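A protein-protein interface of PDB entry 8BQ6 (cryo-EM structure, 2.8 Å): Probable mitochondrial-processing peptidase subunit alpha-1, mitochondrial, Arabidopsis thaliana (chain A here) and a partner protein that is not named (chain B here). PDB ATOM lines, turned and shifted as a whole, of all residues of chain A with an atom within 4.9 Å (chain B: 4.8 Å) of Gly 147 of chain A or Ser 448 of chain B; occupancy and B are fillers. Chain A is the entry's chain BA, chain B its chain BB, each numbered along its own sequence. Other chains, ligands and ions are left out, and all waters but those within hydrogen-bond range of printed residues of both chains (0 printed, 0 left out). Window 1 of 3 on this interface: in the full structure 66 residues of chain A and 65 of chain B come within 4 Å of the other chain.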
ATOM      1  N   ILE A 143     -29.832 -21.220  17.814  1.00  0.00           N
ATOM      2  CA  ILE A 143     -30.000 -22.545  17.225  1.00  0.00           C
ATOM      3  C   ILE A 143     -28.923 -22.814  16.184  1.00  0.00           C
ATOM      4  O   ILE A 143     -28.377 -23.922  16.106  1.00  0.00           O
ATOM      5  CB  ILE A 143     -31.417 -22.677  16.640  1.00  0.00           C
ATOM      6  CG1 ILE A 143     -32.445 -22.712  17.773  1.00  0.00           C
ATOM      7  CG2 ILE A 143     -31.527 -23.891  15.732  1.00  0.00           C
ATOM      8  CD1 ILE A 143     -33.805 -22.236  17.371  1.00  0.00           C
ATOM      9  N   GLU A 144     -28.594 -21.808  15.373  1.00  0.00           N
ATOM     10  CA  GLU A 144     -27.552 -21.967  14.366  1.00  0.00           C
ATOM     11  C   GLU A 144     -26.188 -22.217  14.997  1.00  0.00           C
ATOM     12  O   GLU A 144     -25.387 -22.983  14.451  1.00  0.00           O
ATOM     13  CB  GLU A 144     -27.497 -20.727  13.482  1.00  0.00           C
ATOM     14  CG  GLU A 144     -28.544 -20.696  12.401  1.00  0.00           C
ATOM     15  CD  GLU A 144     -27.962 -20.262  11.081  1.00  0.00           C
ATOM     16  OE1 GLU A 144     -27.451 -19.127  11.008  1.00  0.00           O
ATOM     17  OE2 GLU A 144     -27.993 -21.057  10.123  1.00  0.00           O
ATOM     18  N   ALA A 145     -25.913 -21.577  16.136  1.00  0.00           N
ATOM     19  CA  ALA A 145     -24.613 -21.707  16.790  1.00  0.00           C
ATOM     20  C   ALA A 145     -24.336 -23.133  17.249  1.00  0.00           C
ATOM     21  O   ALA A 145     -23.170 -23.523  17.370  1.00  0.00           O
ATOM     22  CB  ALA A 145     -24.529 -20.753  17.980  1.00  0.00           C
ATOM     23  N   ILE A 146     -25.373 -23.920  17.524  1.00  0.00           N
ATOM     24  CA  ILE A 146     -25.182 -25.304  17.931  1.00  0.00           C
ATOM     25  C   ILE A 146     -25.508 -26.275  16.803  1.00  0.00           C
ATOM     26  O   ILE A 146     -25.568 -27.487  17.031  1.00  0.00           O
ATOM     27  CB  ILE A 146     -25.988 -25.629  19.198  1.00  0.00           C
ATOM     28  CG1 ILE A 146     -27.486 -25.496  18.941  1.00  0.00           C
ATOM     29  CG2 ILE A 146     -25.572 -24.716  20.336  1.00  0.00           C
ATOM     30  CD1 ILE A 146     -28.302 -26.556  19.614  1.00  0.00           C
ATOM     31  N   GLY A 147     -25.703 -25.773  15.586  1.00  0.00           N
ATOM     32  CA  GLY A 147     -26.001 -26.642  14.462  1.00  0.00           C
ATOM     33  C   GLY A 147     -27.343 -27.327  14.556  1.00  0.00           C
ATOM     34  O   GLY A 147     -27.510 -28.428  14.025  1.00  0.00           O
ATOM     35  N   GLY A 148     -28.310 -26.701  15.224  1.00  0.00           N
ATOM     36  CA  GLY A 148     -29.610 -27.307  15.404  1.00  0.00           C
ATOM     37  C   GLY A 148     -30.562 -27.052  14.252  1.00  0.00           C
ATOM     38  O   GLY A 148     -30.302 -26.257  13.353  1.00  0.00           O
ATOM     39  N   ASN A 149     -31.682 -27.768  14.293  1.00  0.00           N
ATOM     40  CA  ASN A 149     -32.791 -27.596  13.367  1.00  0.00           C
ATOM     41  C   ASN A 149     -34.086 -27.670  14.153  1.00  0.00           C
ATOM     42  O   ASN A 149     -34.224 -28.501  15.053  1.00  0.00           O
ATOM     43  CB  ASN A 149     -32.799 -28.666  12.273  1.00  0.00           C
ATOM     44  CG  ASN A 149     -31.425 -28.953  11.733  1.00  0.00           C
ATOM     45  OD1 ASN A 149     -30.997 -28.356  10.746  1.00  0.00           O
ATOM     46  ND2 ASN A 149     -30.709 -29.852  12.393  1.00  0.00           N
ATOM     47  N   ASP A 164     -33.522 -30.593  16.836  1.00  0.00           N
ATOM     48  CA  ASP A 164     -32.597 -31.683  16.556  1.00  0.00           C
ATOM     49  C   ASP A 164     -31.174 -31.142  16.541  1.00  0.00           C
ATOM     50  O   ASP A 164     -30.873 -30.215  15.784  1.00  0.00           O
ATOM     51  CB  ASP A 164     -32.924 -32.330  15.209  1.00  0.00           C
ATOM     52  CG  ASP A 164     -34.073 -33.309  15.300  1.00  0.00           C
ATOM     53  OD1 ASP A 164     -35.236 -32.870  15.194  1.00  0.00           O
ATOM     54  OD2 ASP A 164     -33.819 -34.517  15.466  1.00  0.00           O
ATOM     55  N   ALA A 165     -30.301 -31.725  17.359  1.00  0.00           N
ATOM     56  CA  ALA A 165     -28.912 -31.292  17.423  1.00  0.00           C
ATOM     57  C   ALA A 165     -28.080 -32.404  18.049  1.00  0.00           C
ATOM     58  O   ALA A 165     -28.590 -33.476  18.386  1.00  0.00           O
ATOM     59  CB  ALA A 165     -28.771 -29.981  18.204  1.00  0.00           C
ATOM     60  N   LEU A 166     -26.784 -32.140  18.191  1.00  0.00           N
ATOM     61  CA  LEU A 166     -25.877 -33.081  18.832  1.00  0.00           C
ATOM     62  C   LEU A 166     -26.191 -33.190  20.322  1.00  0.00           C
ATOM     63  O   LEU A 166     -26.692 -32.249  20.943  1.00  0.00           O
ATOM     64  CB  LEU A 166     -24.427 -32.637  18.627  1.00  0.00           C
ATOM     65  CG  LEU A 166     -23.865 -32.728  17.203  1.00  0.00           C
ATOM     66  CD1 LEU A 166     -22.352 -32.582  17.205  1.00  0.00           C
ATOM     67  CD2 LEU A 166     -24.278 -34.025  16.515  1.00  0.00           C
ATOM     68  N   ASN B 444     -19.669 -25.611  12.754  1.00  0.00           N
ATOM     69  CA  ASN B 444     -20.585 -26.287  13.669  1.00  0.00           C
ATOM     70  C   ASN B 444     -21.799 -26.835  12.933  1.00  0.00           C
ATOM     71  O   ASN B 444     -22.287 -27.925  13.249  1.00  0.00           O
ATOM     72  CB  ASN B 444     -21.031 -25.331  14.772  1.00  0.00           C
ATOM     73  CG  ASN B 444     -19.971 -25.121  15.824  1.00  0.00           C
ATOM     74  OD1 ASN B 444     -19.008 -25.881  15.915  1.00  0.00           O
ATOM     75  ND2 ASN B 444     -20.144 -24.087  16.632  1.00  0.00           N
ATOM     76  N   GLN B 445     -22.319 -26.076  11.969  1.00  0.00           N
ATOM     77  CA  GLN B 445     -23.477 -26.534  11.214  1.00  0.00           C
ATOM     78  C   GLN B 445     -23.129 -27.732  10.342  1.00  0.00           C
ATOM     79  O   GLN B 445     -23.936 -28.656  10.193  1.00  0.00           O
ATOM     80  CB  GLN B 445     -24.024 -25.395  10.364  1.00  0.00           C
ATOM     81  CG  GLN B 445     -24.703 -24.318  11.164  1.00  0.00           C
ATOM     82  CD  GLN B 445     -25.121 -23.161  10.302  1.00  0.00           C
ATOM     83  OE1 GLN B 445     -24.287 -22.475   9.716  1.00  0.00           O
ATOM     84  NE2 GLN B 445     -26.421 -22.947  10.200  1.00  0.00           N
ATOM     85  N   LEU B 446     -21.935 -27.727   9.748  1.00  0.00           N
ATOM     86  CA  LEU B 446     -21.519 -28.844   8.909  1.00  0.00           C
ATOM     87  C   LEU B 446     -21.279 -30.103   9.735  1.00  0.00           C
ATOM     88  O   LEU B 446     -21.685 -31.199   9.335  1.00  0.00           O
ATOM     89  CB  LEU B 446     -20.265 -28.464   8.127  1.00  0.00           C
ATOM     90  CG  LEU B 446     -19.641 -29.567   7.280  1.00  0.00           C
ATOM     91  CD1 LEU B 446     -20.613 -30.021   6.214  1.00  0.00           C
ATOM     92  CD2 LEU B 446     -18.360 -29.068   6.656  1.00  0.00           C
ATOM     93  N   LYS B 447     -20.627 -29.966  10.891  1.00  0.00           N
ATOM     94  CA  LYS B 447     -20.416 -31.118  11.763  1.00  0.00           C
ATOM     95  C   LYS B 447     -21.738 -31.718  12.208  1.00  0.00           C
ATOM     96  O   LYS B 447     -21.877 -32.942  12.310  1.00  0.00           O
ATOM     97  CB  LYS B 447     -19.597 -30.717  12.983  1.00  0.00           C
ATOM     98  CG  LYS B 447     -18.187 -30.333  12.682  1.00  0.00           C
ATOM     99  CD  LYS B 447     -17.359 -30.482  13.919  1.00  0.00           C
ATOM    100  CE  LYS B 447     -17.063 -29.141  14.537  1.00  0.00           C
ATOM    101  NZ  LYS B 447     -16.010 -29.298  15.567  1.00  0.00           N
ATOM    102  N   SER B 448     -22.718 -30.865  12.502  1.00  0.00           N
ATOM    103  CA  SER B 448     -24.007 -31.361  12.965  1.00  0.00           C
ATOM    104  C   SER B 448     -24.786 -32.029  11.838  1.00  0.00           C
ATOM    105  O   SER B 448     -25.418 -33.070  12.046  1.00  0.00           O
ATOM    106  CB  SER B 448     -24.816 -30.220  13.572  1.00  0.00           C
ATOM    107  OG  SER B 448     -26.144 -30.634  13.823  1.00  0.00           O
ATOM    108  N   SER B 449     -24.759 -31.444  10.639  1.00  0.00           N
ATOM    109  CA  SER B 449     -25.565 -31.980   9.548  1.00  0.00           C
ATOM    110  C   SER B 449     -25.029 -33.313   9.050  1.00  0.00           C
ATOM    111  O   SER B 449     -25.810 -34.181   8.646  1.00  0.00           O
ATOM    112  CB  SER B 449     -25.631 -30.980   8.398  1.00  0.00           C
ATOM    113  OG  SER B 449     -24.447 -31.027   7.628  1.00  0.00           O
ATOM    114  N   LEU B 450     -23.710 -33.486   9.074  1.00  0.00           N
ATOM    115  CA  LEU B 450     -23.088 -34.725   8.544  1.00  0.00           C
ATOM    116  C   LEU B 450     -23.395 -35.913   9.460  1.00  0.00           C
ATOM    117  O   LEU B 450     -23.256 -37.049   8.986  1.00  0.00           O
ATOM    118  CB  LEU B 450     -21.578 -34.502   8.455  1.00  0.00           C
ATOM    119  CG  LEU B 450     -21.085 -33.805   7.191  1.00  0.00           C
ATOM    120  CD1 LEU B 450     -19.567 -33.717   7.187  1.00  0.00           C
ATOM    121  CD2 LEU B 450     -21.586 -34.516   5.945  1.00  0.00           C
ATOM    122  N   LEU B 451     -23.789 -35.668  10.710  1.00  0.00           N
ATOM    123  CA  LEU B 451     -24.012 -36.777  11.673  1.00  0.00           C
ATOM    124  C   LEU B 451     -25.503 -36.934  11.986  1.00  0.00           C
ATOM    125  O   LEU B 451     -25.888 -38.022  12.456  1.00  0.00           O
ATOM    126  CB  LEU B 451     -23.222 -36.473  12.943  1.00  0.00           C
ATOM    127  CG  LEU B 451     -22.319 -37.602  13.423  1.00  0.00           C
ATOM    128  CD1 LEU B 451     -21.478 -38.139  12.276  1.00  0.00           C
ATOM    129  CD2 LEU B 451     -21.440 -37.122  14.560  1.00  0.00           C
ATOM    130  N   LEU B 452     -26.300 -35.895  11.743  1.00  0.00           N
ATOM    131  CA  LEU B 452     -27.765 -35.962  11.976  1.00  0.00           C
ATOM    132  C   LEU B 452     -28.440 -36.574  10.751  1.00  0.00           C
ATOM    133  O   LEU B 452     -29.607 -36.972  10.881  1.00  0.00           O
ATOM    134  CB  LEU B 452     -28.289 -34.547  12.231  1.00  0.00           C
ATOM    135  CG  LEU B 452     -28.721 -34.229  13.659  1.00  0.00           C
ATOM    136  CD1 LEU B 452     -27.518 -33.969  14.548  1.00  0.00           C
ATOM    137  CD2 LEU B 452     -29.637 -33.024  13.663  1.00  0.00           C
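Of the 10 printed residues of chain A, 7 touch a printed residue of chain B.
Hydrophobic or aromatic side chains of chain A within 4 Å of the printed part of chain B: Leu 166.
Of the 9 printed residues of chain B, 4 touch a printed residue of chain A.
Among the printed residues, 7 pairs touch across the chains.
Among the printed residues, no Asp or Glu carboxylate lies within 4 Å of a Lys or Arg side-chain nitrogen of the other chain.
N of Asp 164 of chain A lies within hydrogen-bond range of O of Asn 149 of chain A (2.8 Å).
OE2 of Glu 144 of chain A sits at hydrogen-bond distance from NE2 of Gln 445 of chain B (2.5 Å).
The backbone carbonyl oxygen of Gly 147 of chain A lies within hydrogen-bond range of the side-chain hydroxyl of Ser 448 of chain B, 2.6 Å away.
The backbone carbonyl oxygen (O) of Ala 145 of chain A is in hydrogen-bond range of the side-chain amide nitrogen (ND2) of Asn 444 of chain B, at 3.2 Å.
Printed residues of chain B within 4 Å of Glu 144 of chain A: Gln 445 (2.5 Å).
Ile 146 of chain A touches none of the printed residues of chain B.
Gly 147 of chain A touches just one residue of chain B: Ser 448.
Gly 148 of chain A touches none of the printed residues of chain B.
Printed residues of chain B within 4 Å of Asp 164 of chain A: Leu 452.
Printed residues of chain B within 4 Å of Leu 166 of chain A: Leu 452 (3.8 Å).
Of the printed residues of chain A, Asn 444 of chain B touches Ala 145.
Printed residues of chain A within 4 Å of Gln 445 of chain B: Glu 144 (2.5 Å).
Ser 448 of chain B touches just one residue of chain A: Gly 147 (2.6 Å).
The nearest printed residue of chain A that does not touch Ser 448 of chain B is Leu 166 of chain A (4.4 Å).
The nearest printed residue of chain A that does not touch Leu 452 of chain B is Gly 147 of chain A (5.1 Å).
Asn 149 of chain A touches Leu 452 of chain B.
Asp 164 of chain A touches Leu 452 of chain B (CB to CD2, 3.7 Å).
Ala 165 of chain A touches Leu 452 of chain B.
Leu 166 of chain A touches Leu 452 of chain B (CD2 to CD1, 3.8 Å).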
